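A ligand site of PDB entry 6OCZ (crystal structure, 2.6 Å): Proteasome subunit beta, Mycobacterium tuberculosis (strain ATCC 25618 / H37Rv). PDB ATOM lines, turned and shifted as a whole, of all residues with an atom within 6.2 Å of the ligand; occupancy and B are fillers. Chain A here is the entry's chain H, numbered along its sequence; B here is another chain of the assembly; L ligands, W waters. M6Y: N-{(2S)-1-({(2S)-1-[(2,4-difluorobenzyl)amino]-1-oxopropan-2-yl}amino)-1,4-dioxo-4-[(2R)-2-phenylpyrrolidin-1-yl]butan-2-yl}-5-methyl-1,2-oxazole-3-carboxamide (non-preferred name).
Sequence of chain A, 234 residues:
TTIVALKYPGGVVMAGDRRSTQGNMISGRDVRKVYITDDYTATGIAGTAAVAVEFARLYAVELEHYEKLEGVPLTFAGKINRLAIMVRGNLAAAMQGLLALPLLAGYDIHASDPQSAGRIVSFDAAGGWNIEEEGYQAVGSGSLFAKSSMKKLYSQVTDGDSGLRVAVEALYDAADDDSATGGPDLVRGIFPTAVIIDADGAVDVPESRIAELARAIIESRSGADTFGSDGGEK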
ATOM      1  N   THR A   1     -17.371 -12.210  -2.612  1.00  0.00           N
ATOM      2  CA  THR A   1     -16.430 -11.115  -2.393  1.00  0.00           C
ATOM      3  C   THR A   1     -15.968 -11.056  -0.944  1.00  0.00           C
ATOM      4  O   THR A   1     -16.735 -11.316  -0.026  1.00  0.00           O
ATOM      5  CB  THR A   1     -17.044  -9.740  -2.786  1.00  0.00           C
ATOM      6  OG1 THR A   1     -17.169  -9.657  -4.208  1.00  0.00           O
ATOM      7  CG2 THR A   1     -16.185  -8.593  -2.282  1.00  0.00           C
ATOM      8  N   ILE A   3     -13.288  -8.174   1.225  1.00  0.00           N
ATOM      9  CA  ILE A   3     -12.339  -7.068   1.265  1.00  0.00           C
ATOM     10  C   ILE A   3     -11.856  -6.931   2.702  1.00  0.00           C
ATOM     11  O   ILE A   3     -12.659  -6.996   3.644  1.00  0.00           O
ATOM     12  CB  ILE A   3     -12.978  -5.748   0.782  1.00  0.00           C
ATOM     13  CG1 ILE A   3     -13.744  -5.954  -0.522  1.00  0.00           C
ATOM     14  CG2 ILE A   3     -11.902  -4.685   0.596  1.00  0.00           C
ATOM     15  CD1 ILE A   3     -12.933  -5.725  -1.773  1.00  0.00           C
ATOM     16  N   ARG A  19     -12.789 -12.801  -7.563  1.00  0.00           N
ATOM     17  CA  ARG A  19     -13.860 -13.619  -8.101  1.00  0.00           C
ATOM     18  C   ARG A  19     -15.128 -12.819  -8.377  1.00  0.00           C
ATOM     19  O   ARG A  19     -15.466 -11.880  -7.646  1.00  0.00           O
ATOM     20  CB  ARG A  19     -14.187 -14.768  -7.136  1.00  0.00           C
ATOM     21  CG  ARG A  19     -15.459 -15.529  -7.505  1.00  0.00           C
ATOM     22  CD  ARG A  19     -15.493 -16.881  -6.845  1.00  0.00           C
ATOM     23  NE  ARG A  19     -14.431 -17.745  -7.336  1.00  0.00           N
ATOM     24  CZ  ARG A  19     -14.196 -18.980  -6.886  1.00  0.00           C
ATOM     25  NH1 ARG A  19     -14.946 -19.491  -5.925  1.00  0.00           N
ATOM     26  NH2 ARG A  19     -13.206 -19.689  -7.387  1.00  0.00           N
ATOM     27  N   SER A  20     -15.812 -13.220  -9.441  1.00  0.00           N
ATOM     28  CA  SER A  20     -17.089 -12.661  -9.856  1.00  0.00           C
ATOM     29  C   SER A  20     -18.059 -13.814 -10.088  1.00  0.00           C
ATOM     30  O   SER A  20     -17.707 -14.794 -10.749  1.00  0.00           O
ATOM     31  CB  SER A  20     -16.925 -11.834 -11.134  1.00  0.00           C
ATOM     32  OG  SER A  20     -18.171 -11.296 -11.550  1.00  0.00           O
ATOM     33  N   THR A  21     -19.275 -13.731  -9.550  1.00  0.00           N
ATOM     34  CA  THR A  21     -20.261 -14.784  -9.721  1.00  0.00           C
ATOM     35  C   THR A  21     -21.555 -14.246 -10.295  1.00  0.00           C
ATOM     36  O   THR A  21     -21.875 -13.061 -10.170  1.00  0.00           O
ATOM     37  CB  THR A  21     -20.573 -15.498  -8.395  1.00  0.00           C
ATOM     38  OG1 THR A  21     -20.760 -14.537  -7.352  1.00  0.00           O
ATOM     39  CG2 THR A  21     -19.460 -16.465  -8.029  1.00  0.00           C
ATOM     40  N   GLN A  22     -22.298 -15.134 -10.948  1.00  0.00           N
ATOM     41  CA  GLN A  22     -23.701 -14.947 -11.316  1.00  0.00           C
ATOM     42  C   GLN A  22     -24.454 -16.100 -10.660  1.00  0.00           C
ATOM     43  O   GLN A  22     -24.639 -17.161 -11.258  1.00  0.00           O
ATOM     44  CB  GLN A  22     -23.893 -14.934 -12.824  1.00  0.00           C
ATOM     45  CG  GLN A  22     -23.961 -13.555 -13.442  1.00  0.00           C
ATOM     46  CD  GLN A  22     -24.390 -13.600 -14.890  1.00  0.00           C
ATOM     47  OE1 GLN A  22     -24.777 -14.644 -15.405  1.00  0.00           O
ATOM     48  NE2 GLN A  22     -24.327 -12.449 -15.563  1.00  0.00           N
ATOM     49  N   GLY A  23     -24.873 -15.883  -9.409  1.00  0.00           N
ATOM     50  CA  GLY A  23     -25.397 -16.970  -8.606  1.00  0.00           C
ATOM     51  C   GLY A  23     -24.296 -17.945  -8.241  1.00  0.00           C
ATOM     52  O   GLY A  23     -23.315 -17.571  -7.607  1.00  0.00           O
ATOM     53  N   SER A  27     -18.259 -16.060 -13.040  1.00  0.00           N
ATOM     54  CA  SER A  27     -18.220 -15.191 -14.200  1.00  0.00           C
ATOM     55  C   SER A  27     -16.964 -14.334 -14.281  1.00  0.00           C
ATOM     56  O   SER A  27     -16.769 -13.642 -15.292  1.00  0.00           O
ATOM     57  CB  SER A  27     -19.457 -14.279 -14.237  1.00  0.00           C
ATOM     58  OG  SER A  27     -19.636 -13.612 -12.995  1.00  0.00           O
ATOM     59  N   GLY A  28     -16.103 -14.366 -13.269  1.00  0.00           N
ATOM     60  CA  GLY A  28     -14.871 -13.598 -13.321  1.00  0.00           C
ATOM     61  C   GLY A  28     -13.830 -14.183 -12.392  1.00  0.00           C
ATOM     62  O   GLY A  28     -14.151 -14.695 -11.312  1.00  0.00           O
ATOM     63  N   VAL A  31     -11.056 -10.020 -11.309  1.00  0.00           N
ATOM     64  CA  VAL A  31     -11.705  -8.752 -11.017  1.00  0.00           C
ATOM     65  C   VAL A  31     -10.869  -7.972 -10.018  1.00  0.00           C
ATOM     66  O   VAL A  31     -10.350  -8.525  -9.032  1.00  0.00           O
ATOM     67  CB  VAL A  31     -13.129  -9.006 -10.483  1.00  0.00           C
ATOM     68  CG1 VAL A  31     -13.853  -7.696 -10.253  1.00  0.00           C
ATOM     69  CG2 VAL A  31     -13.891  -9.900 -11.441  1.00  0.00           C
ATOM     70  N   ARG A  32     -10.708  -6.679 -10.276  1.00  0.00           N
ATOM     71  CA  ARG A  32     -10.013  -5.776  -9.355  1.00  0.00           C
ATOM     72  C   ARG A  32     -11.065  -5.032  -8.538  1.00  0.00           C
ATOM     73  O   ARG A  32     -11.883  -4.287  -9.093  1.00  0.00           O
ATOM     74  CB  ARG A  32      -9.103  -4.814 -10.112  1.00  0.00           C
ATOM     75  CG  ARG A  32      -7.967  -5.540 -10.849  1.00  0.00           C
ATOM     76  CD  ARG A  32      -6.884  -4.609 -11.370  1.00  0.00           C
ATOM     77  NE  ARG A  32      -5.829  -5.365 -12.064  1.00  0.00           N
ATOM     78  CZ  ARG A  32      -4.701  -5.776 -11.491  1.00  0.00           C
ATOM     79  NH1 ARG A  32      -4.466  -5.500 -10.215  1.00  0.00           N
ATOM     80  NH2 ARG A  32      -3.810  -6.471 -12.200  1.00  0.00           N
ATOM     81  N   LYS A  33     -11.050  -5.245  -7.224  1.00  0.00           N
ATOM     82  CA  LYS A  33     -12.058  -4.710  -6.326  1.00  0.00           C
ATOM     83  C   LYS A  33     -11.541  -3.642  -5.383  1.00  0.00           C
ATOM     84  O   LYS A  33     -12.348  -3.038  -4.670  1.00  0.00           O
ATOM     85  CB  LYS A  33     -12.692  -5.845  -5.497  1.00  0.00           C
ATOM     86  CG  LYS A  33     -13.244  -6.984  -6.325  1.00  0.00           C
ATOM     87  CD  LYS A  33     -13.868  -8.055  -5.448  1.00  0.00           C
ATOM     88  CE  LYS A  33     -14.316  -9.235  -6.280  1.00  0.00           C
ATOM     89  NZ  LYS A  33     -14.977 -10.277  -5.447  1.00  0.00           N
ATOM     90  N   TYR A  35      -9.452  -0.122  -5.200  1.00  0.00           N
ATOM     91  CA  TYR A  35      -9.021   0.979  -6.053  1.00  0.00           C
ATOM     92  C   TYR A  35      -8.344   2.054  -5.225  1.00  0.00           C
ATOM     93  O   TYR A  35      -8.775   2.353  -4.102  1.00  0.00           O
ATOM     94  CB  TYR A  35     -10.212   1.592  -6.813  1.00  0.00           C
ATOM     95  CG  TYR A  35     -10.851   0.664  -7.813  1.00  0.00           C
ATOM     96  CD1 TYR A  35     -10.246   0.402  -9.046  1.00  0.00           C
ATOM     97  CD2 TYR A  35     -12.079   0.055  -7.541  1.00  0.00           C
ATOM     98  CE1 TYR A  35     -10.830  -0.449  -9.963  1.00  0.00           C
ATOM     99  CE2 TYR A  35     -12.668  -0.798  -8.472  1.00  0.00           C
ATOM    100  CZ  TYR A  35     -12.042  -1.035  -9.678  1.00  0.00           C
ATOM    101  OH  TYR A  35     -12.635  -1.886 -10.592  1.00  0.00           O
ATOM    102  N   ILE A  45     -14.977  -2.462  -2.570  1.00  0.00           N
ATOM    103  CA  ILE A  45     -16.433  -2.491  -2.629  1.00  0.00           C
ATOM    104  C   ILE A  45     -16.913  -3.919  -2.864  1.00  0.00           C
ATOM    105  O   ILE A  45     -16.374  -4.622  -3.712  1.00  0.00           O
ATOM    106  CB  ILE A  45     -16.957  -1.553  -3.728  1.00  0.00           C
ATOM    107  CG1 ILE A  45     -16.128  -0.256  -3.745  1.00  0.00           C
ATOM    108  CG2 ILE A  45     -18.432  -1.244  -3.505  1.00  0.00           C
ATOM    109  CD1 ILE A  45     -16.665   0.798  -4.664  1.00  0.00           C
ATOM    110  N   ALA A  46     -17.943  -4.319  -2.117  1.00  0.00           N
ATOM    111  CA  ALA A  46     -18.597  -5.612  -2.289  1.00  0.00           C
ATOM    112  C   ALA A  46     -20.020  -5.394  -2.799  1.00  0.00           C
ATOM    113  O   ALA A  46     -20.677  -4.424  -2.439  1.00  0.00           O
ATOM    114  CB  ALA A  46     -18.628  -6.389  -0.977  1.00  0.00           C
ATOM    115  N   GLY A  47     -20.481  -6.313  -3.639  1.00  0.00           N
ATOM    116  CA  GLY A  47     -21.862  -6.253  -4.104  1.00  0.00           C
ATOM    117  C   GLY A  47     -22.026  -6.353  -5.608  1.00  0.00           C
ATOM    118  O   GLY A  47     -21.256  -7.043  -6.271  1.00  0.00           O
ATOM    119  N   THR A  48     -23.044  -5.686  -6.144  1.00  0.00           N
ATOM    120  CA  THR A  48     -23.287  -5.706  -7.583  1.00  0.00           C
ATOM    121  C   THR A  48     -22.138  -5.009  -8.303  1.00  0.00           C
ATOM    122  O   THR A  48     -21.835  -3.847  -8.024  1.00  0.00           O
ATOM    123  CB  THR A  48     -24.619  -5.020  -7.903  1.00  0.00           C
ATOM    124  OG1 THR A  48     -25.673  -5.643  -7.169  1.00  0.00           O
ATOM    125  CG2 THR A  48     -24.926  -5.111  -9.392  1.00  0.00           C
ATOM    126  N   ALA A  49     -21.511  -5.735  -9.227  1.00  0.00           N
ATOM    127  CA  ALA A  49     -20.279  -5.251  -9.842  1.00  0.00           C
ATOM    128  C   ALA A  49     -20.469  -3.876 -10.473  1.00  0.00           C
ATOM    129  O   ALA A  49     -19.704  -2.946 -10.193  1.00  0.00           O
ATOM    130  CB  ALA A  49     -19.783  -6.260 -10.883  1.00  0.00           C
ATOM    131  N   ALA A  50     -21.475  -3.733 -11.346  1.00  0.00           N
ATOM    132  CA  ALA A  50     -21.701  -2.455 -12.003  1.00  0.00           C
ATOM    133  C   ALA A  50     -21.765  -1.318 -10.993  1.00  0.00           C
ATOM    134  O   ALA A  50     -21.165  -0.249 -11.196  1.00  0.00           O
ATOM    135  CB  ALA A  50     -22.988  -2.508 -12.832  1.00  0.00           C
ATOM    136  N   ALA A  52     -20.535  -1.312  -7.837  1.00  0.00           N
ATOM    137  CA  ALA A  52     -19.270  -1.134  -7.139  1.00  0.00           C
ATOM    138  C   ALA A  52     -18.271  -0.340  -7.983  1.00  0.00           C
ATOM    139  O   ALA A  52     -17.634   0.602  -7.503  1.00  0.00           O
ATOM    140  CB  ALA A  52     -18.678  -2.488  -6.749  1.00  0.00           C
ATOM    141  N   VAL A  53     -18.138  -0.714  -9.264  1.00  0.00           N
ATOM    142  CA  VAL A  53     -17.256   0.004 -10.183  1.00  0.00           C
ATOM    143  C   VAL A  53     -17.701   1.453 -10.307  1.00  0.00           C
ATOM    144  O   VAL A  53     -16.894   2.385 -10.227  1.00  0.00           O
ATOM    145  CB  VAL A  53     -17.219  -0.702 -11.541  1.00  0.00           C
ATOM    146  CG1 VAL A  53     -16.453   0.131 -12.553  1.00  0.00           C
ATOM    147  CG2 VAL A  53     -16.594  -2.090 -11.402  1.00  0.00           C
ATOM    148  N   GLY A  97     -31.911  -4.879  -5.389  1.00  0.00           N
ATOM    149  CA  GLY A  97     -30.882  -5.799  -5.821  1.00  0.00           C
ATOM    150  C   GLY A  97     -29.629  -5.174  -6.395  1.00  0.00           C
ATOM    151  O   GLY A  97     -28.773  -5.907  -6.910  1.00  0.00           O
ATOM    152  N   LEU A  98     -29.501  -3.860  -6.345  1.00  0.00           N
ATOM    153  CA  LEU A  98     -28.265  -3.207  -6.771  1.00  0.00           C
ATOM    154  C   LEU A  98     -27.507  -2.699  -5.552  1.00  0.00           C
ATOM    155  O   LEU A  98     -27.177  -1.513  -5.462  1.00  0.00           O
ATOM    156  CB  LEU A  98     -28.556  -2.081  -7.757  1.00  0.00           C
ATOM    157  CG  LEU A  98     -29.369  -2.500  -8.991  1.00  0.00           C
ATOM    158  CD1 LEU A  98     -29.608  -1.323  -9.927  1.00  0.00           C
ATOM    159  CD2 LEU A  98     -28.679  -3.629  -9.730  1.00  0.00           C
ATOM    160  N   LEU B  91     -32.474  -1.051 -18.145  1.00  0.00           N
ATOM    161  CA  LEU B  91     -32.675  -2.068 -17.117  1.00  0.00           C
ATOM    162  C   LEU B  91     -34.145  -2.241 -16.768  1.00  0.00           C
ATOM    163  O   LEU B  91     -34.605  -3.377 -16.586  1.00  0.00           O
ATOM    164  CB  LEU B  91     -31.871  -1.720 -15.870  1.00  0.00           C
ATOM    165  CG  LEU B  91     -32.086  -2.730 -14.737  1.00  0.00           C
ATOM    166  CD1 LEU B  91     -31.739  -4.145 -15.191  1.00  0.00           C
ATOM    167  CD2 LEU B  91     -31.291  -2.367 -13.489  1.00  0.00           C
ATOM    168  N   SER B 122     -17.546  -8.118 -22.096  1.00  0.00           N
ATOM    169  CA  SER B 122     -18.872  -8.684 -21.862  1.00  0.00           C
ATOM    170  C   SER B 122     -19.646  -7.840 -20.860  1.00  0.00           C
ATOM    171  O   SER B 122     -19.056  -7.150 -20.021  1.00  0.00           O
ATOM    172  CB  SER B 122     -18.783 -10.151 -21.377  1.00  0.00           C
ATOM    173  OG  SER B 122     -18.073 -10.257 -20.160  1.00  0.00           O
ATOM    174  N   PHE B 123     -20.968  -7.895 -20.958  1.00  0.00           N
ATOM    175  CA  PHE B 123     -21.850  -6.996 -20.220  1.00  0.00           C
ATOM    176  C   PHE B 123     -22.973  -7.776 -19.536  1.00  0.00           C
ATOM    177  O   PHE B 123     -23.356  -8.861 -19.979  1.00  0.00           O
ATOM    178  CB  PHE B 123     -22.458  -5.944 -21.157  1.00  0.00           C
ATOM    179  CG  PHE B 123     -21.441  -5.037 -21.795  1.00  0.00           C
ATOM    180  CD1 PHE B 123     -20.721  -5.446 -22.906  1.00  0.00           C
ATOM    181  CD2 PHE B 123     -21.208  -3.760 -21.292  1.00  0.00           C
ATOM    182  CE1 PHE B 123     -19.797  -4.605 -23.499  1.00  0.00           C
ATOM    183  CE2 PHE B 123     -20.293  -2.919 -21.881  1.00  0.00           C
ATOM    184  CZ  PHE B 123     -19.583  -3.341 -22.987  1.00  0.00           C
ATOM    185  N   ASP B 124     -23.497  -7.199 -18.463  1.00  0.00           N
ATOM    186  CA  ASP B 124     -24.664  -7.738 -17.781  1.00  0.00           C
ATOM    187  C   ASP B 124     -25.790  -6.701 -17.794  1.00  0.00           C
ATOM    188  O   ASP B 124     -25.591  -5.543 -18.161  1.00  0.00           O
ATOM    189  CB  ASP B 124     -24.331  -8.166 -16.337  1.00  0.00           C
ATOM    190  CG  ASP B 124     -23.989  -6.988 -15.418  1.00  0.00           C
ATOM    191  OD1 ASP B 124     -24.558  -5.894 -15.575  1.00  0.00           O
ATOM    192  OD2 ASP B 124     -23.135  -7.179 -14.519  1.00  0.00           O
ATOM    193  N   ALA B 125     -26.978  -7.133 -17.378  1.00  0.00           N
ATOM    194  CA  ALA B 125     -28.168  -6.302 -17.536  1.00  0.00           C
ATOM    195  C   ALA B 125     -28.087  -4.996 -16.758  1.00  0.00           C
ATOM    196  O   ALA B 125     -28.790  -4.037 -17.112  1.00  0.00           O
ATOM    197  CB  ALA B 125     -29.413  -7.099 -17.117  1.00  0.00           C
ATOM    198  N   ALA B 126     -27.258  -4.919 -15.726  1.00  0.00           N
ATOM    199  CA  ALA B 126     -27.157  -3.708 -14.911  1.00  0.00           C
ATOM    200  C   ALA B 126     -26.056  -2.764 -15.388  1.00  0.00           C
ATOM    201  O   ALA B 126     -25.710  -1.833 -14.658  1.00  0.00           O
ATOM    202  CB  ALA B 126     -26.932  -4.077 -13.449  1.00  0.00           C
ATOM    203  N   GLY B 127     -25.519  -2.971 -16.579  1.00  0.00           N
ATOM    204  CA  GLY B 127     -24.456  -2.132 -17.088  1.00  0.00           C
ATOM    205  C   GLY B 127     -23.058  -2.552 -16.708  1.00  0.00           C
ATOM    206  O   GLY B 127     -22.089  -1.913 -17.160  1.00  0.00           O
ATOM    207  N   GLY B 128     -22.908  -3.605 -15.908  1.00  0.00           N
ATOM    208  CA  GLY B 128     -21.578  -4.109 -15.613  1.00  0.00           C
ATOM    209  C   GLY B 128     -20.864  -4.547 -16.878  1.00  0.00           C
ATOM    210  O   GLY B 128     -21.449  -5.180 -17.764  1.00  0.00           O
ATOM    211  N   TRP B 129     -19.581  -4.191 -16.975  1.00  0.00           N
ATOM    212  CA  TRP B 129     -18.734  -4.599 -18.089  1.00  0.00           C
ATOM    213  C   TRP B 129     -17.470  -5.232 -17.529  1.00  0.00           C
ATOM    214  O   TRP B 129     -16.988  -4.861 -16.460  1.00  0.00           O
ATOM    215  CB  TRP B 129     -18.368  -3.412 -18.983  1.00  0.00           C
ATOM    216  CG  TRP B 129     -17.763  -2.288 -18.211  1.00  0.00           C
ATOM    217  CD1 TRP B 129     -18.417  -1.232 -17.651  1.00  0.00           C
ATOM    218  CD2 TRP B 129     -16.386  -2.135 -17.865  1.00  0.00           C
ATOM    219  NE1 TRP B 129     -17.537  -0.414 -16.994  1.00  0.00           N
ATOM    220  CE2 TRP B 129     -16.277  -0.946 -17.111  1.00  0.00           C
ATOM    221  CE3 TRP B 129     -15.226  -2.868 -18.137  1.00  0.00           C
ATOM    222  CZ2 TRP B 129     -15.064  -0.488 -16.608  1.00  0.00           C
ATOM    223  CZ3 TRP B 129     -14.027  -2.411 -17.644  1.00  0.00           C
ATOM    224  CH2 TRP B 129     -13.951  -1.237 -16.891  1.00  0.00           C
ATOM    225  N   ASN B 130     -16.951  -6.218 -18.254  1.00  0.00           N
ATOM    226  CA  ASN B 130     -15.712  -6.883 -17.871  1.00  0.00           C
ATOM    227  C   ASN B 130     -14.890  -7.146 -19.125  1.00  0.00           C
ATOM    228  O   ASN B 130     -15.397  -7.733 -20.093  1.00  0.00           O
ATOM    229  CB  ASN B 130     -15.982  -8.205 -17.132  1.00  0.00           C
ATOM    230  CG  ASN B 130     -14.744  -8.750 -16.452  1.00  0.00           C
ATOM    231  OD1 ASN B 130     -13.995  -8.018 -15.795  1.00  0.00           O
ATOM    232  ND2 ASN B 130     -14.504 -10.053 -16.606  1.00  0.00           N
HETATM  233  C25 M6Y L   1     -27.579  -8.646 -11.899  1.00  0.00           C
HETATM  234  C26 M6Y L   1     -28.367  -7.870 -12.745  1.00  0.00           C
HETATM  235  C27 M6Y L   1     -29.802  -7.420 -12.488  1.00  0.00           C
HETATM  236  O28 M6Y L   1     -27.615  -7.581 -13.820  1.00  0.00           O
HETATM  237  N29 M6Y L   1     -26.387  -8.164 -13.674  1.00  0.00           N
HETATM  238  C24 M6Y L   1     -26.345  -8.813 -12.523  1.00  0.00           C
HETATM  239  C22 M6Y L   1     -25.147  -9.591 -11.978  1.00  0.00           C
HETATM  240  O23 M6Y L   1     -25.302 -10.437 -11.159  1.00  0.00           O
HETATM  241  C13 M6Y L   1     -20.045  -7.986 -16.618  1.00  0.00           C
HETATM  242  C15 M6Y L   1     -18.955  -8.169 -14.581  1.00  0.00           C
HETATM  243  C17 M6Y L   1     -16.985  -9.151 -13.639  1.00  0.00           C
HETATM  244  C20 M6Y L   1     -18.520  -6.913 -14.190  1.00  0.00           C
HETATM  245  C04 M6Y L   1     -22.365  -9.511 -10.533  1.00  0.00           C
HETATM  246  C06 M6Y L   1     -22.689 -10.026 -11.933  1.00  0.00           C
HETATM  247  C07 M6Y L   1     -21.461  -9.793 -12.816  1.00  0.00           C
HETATM  248  C08 M6Y L   1     -21.374 -10.517 -14.153  1.00  0.00           C
HETATM  249  C11 M6Y L   1     -20.665 -10.335 -16.525  1.00  0.00           C
HETATM  250  C12 M6Y L   1     -19.720  -9.337 -17.278  1.00  0.00           C
HETATM  251  C14 M6Y L   1     -20.266  -8.304 -15.321  1.00  0.00           C
HETATM  252  C16 M6Y L   1     -18.186  -9.289 -14.314  1.00  0.00           C
HETATM  253  C18 M6Y L   1     -16.557  -7.900 -13.237  1.00  0.00           C
HETATM  254  C19 M6Y L   1     -17.320  -6.774 -13.516  1.00  0.00           C
HETATM  255  N10 M6Y L   1     -20.806  -9.827 -15.306  1.00  0.00           N
HETATM  256  N21 M6Y L   1     -23.818  -9.295 -12.459  1.00  0.00           N
HETATM  257  O05 M6Y L   1     -22.486  -8.357 -10.274  1.00  0.00           O
HETATM  258  O09 M6Y L   1     -21.749 -11.641 -14.257  1.00  0.00           O
HETATM  259  N03 M6Y L   1     -21.897 -10.454  -9.526  1.00  0.00           N
HETATM  260  C02 M6Y L   1     -21.565 -10.004  -8.182  1.00  0.00           C
HETATM  261  C30 M6Y L   1     -20.035 -10.002  -8.064  1.00  0.00           C
HETATM  262  O31 M6Y L   1     -19.398 -10.901  -8.518  1.00  0.00           O
HETATM  263  C01 M6Y L   1     -22.182 -10.973  -7.184  1.00  0.00           C
HETATM  264  C33 M6Y L   1     -17.878  -8.966  -7.308  1.00  0.00           C
HETATM  265  C34 M6Y L   1     -17.297  -7.579  -7.595  1.00  0.00           C
HETATM  266  C35 M6Y L   1     -16.990  -6.732  -6.533  1.00  0.00           C
HETATM  267  C36 M6Y L   1     -16.456  -5.478  -6.790  1.00  0.00           C
HETATM  268  C37 M6Y L   1     -16.234  -5.068  -8.092  1.00  0.00           C
HETATM  269  C39 M6Y L   1     -16.548  -5.907  -9.145  1.00  0.00           C
HETATM  270  C40 M6Y L   1     -17.072  -7.162  -8.892  1.00  0.00           C
HETATM  271  F38 M6Y L   1     -15.722  -3.835  -8.346  1.00  0.00           F
HETATM  272  F41 M6Y L   1     -17.378  -7.991  -9.926  1.00  0.00           F
HETATM  273  N32 M6Y L   1     -19.333  -8.920  -7.400  1.00  0.00           N
HETATM  274  O   HOH W   1     -23.214  -5.790 -12.126  1.00  0.00           O
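Thr 1 touches the ligand.
O of Arg 19 touches C33 of the ligand, 3.8 Å away.
Val 31 touches the ligand (CG1 to C39, 3.4 Å).
O of Arg 32 touches F38 of the ligand, 3.9 Å away.
CD of Lys 33 touches C35 of the ligand, at 3.6 Å.
O of Ile 45 touches C36 of the ligand, at 3.2 Å.
Thr 48 touches the ligand (CA to O05, 3.9 Å).
CB of Ala 52 touches F38 of the ligand, 3.6 Å away.
Val 53 touches the ligand (CG2 to F38, 3.6 Å).
Ser 122 of chain B touches the ligand (OG to C12, 3.4 Å).
N of Ala 125 of chain B touches O28 of the ligand (3.6 Å).
O of Gly 128 of chain B touches C13 of the ligand, 3.3 Å away.
Trp 129 of chain B touches the ligand (O to C20, 3.4 Å).
Asn 130 of chain B touches the ligand.
The nearest printed residue that does not touch the ligand is Phe 123 of chain B (4.1 Å).
An oxygen (O28) of the ligand lies within hydrogen-bond range of the backbone NH (N) of Ala 126 of chain B.
O of Gly 47 sits at hydrogen-bond distance from N32 of the ligand, at 2.9 Å.
A nitrogen (N21) of the ligand sits at hydrogen-bond distance from the side-chain carboxylate (OD2) of Asp 124 of chain B.
O09 of the ligand is in hydrogen-bond range of NE2 of Gln 22, at 3.0 Å.
The backbone NH (N) of Ala 49 sits at hydrogen-bond distance from an oxygen (O05) of the ligand (3.0 Å).
An oxygen (O31) of the ligand lies close to the side-chain hydroxyl (OG) of Ser 20, 3.3 Å away.
The side-chain hydroxyl (OG) of Ser 27 lies within hydrogen-bond range of an oxygen (O09) of the ligand (3.2 Å).
O31 of the ligand sits at hydrogen-bond distance from N of Thr 21, 3.0 Å away.
O of Thr 21 lies within hydrogen-bond range of N03 of the ligand, at 2.7 Å.
Water W1 lies within hydrogen-bond range of the side-chain carboxylate of Asp 124 of chain B, the backbone NH of Ala 50, an oxygen (O05) of the ligand and the backbone NH of Ala 49.
The backbone NH (N) of Thr 21 lies close to the side-chain hydroxyl (OG) of Ser 27.
N of Ile 45 sits at hydrogen-bond distance from O of Lys 33, at 3.4 Å.
The backbone carbonyl oxygen (O) of Arg 32 sits at hydrogen-bond distance from the side-chain hydroxyl (OH) of Tyr 35, 2.9 Å away.
The backbone NH of Ser 27 is in hydrogen-bond range of the backbone carbonyl oxygen of Ser 20 (2.7 Å).
N of Ser 20 lies within hydrogen-bond range of O of Gly 28.
The side-chain hydroxyl of Thr 1 lies within hydrogen-bond range of the side-chain amino group of Lys 33 (2.6 Å).
The side-chain hydroxyl (OG1) of Thr 48 lies within hydrogen-bond range of the backbone carbonyl oxygen (O) of Gly 97.
The side-chain carboxylate (OD1) of Asp 124 of chain B lies within hydrogen-bond range of the backbone NH (N) of Gly 127 of chain B (3.2 Å).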
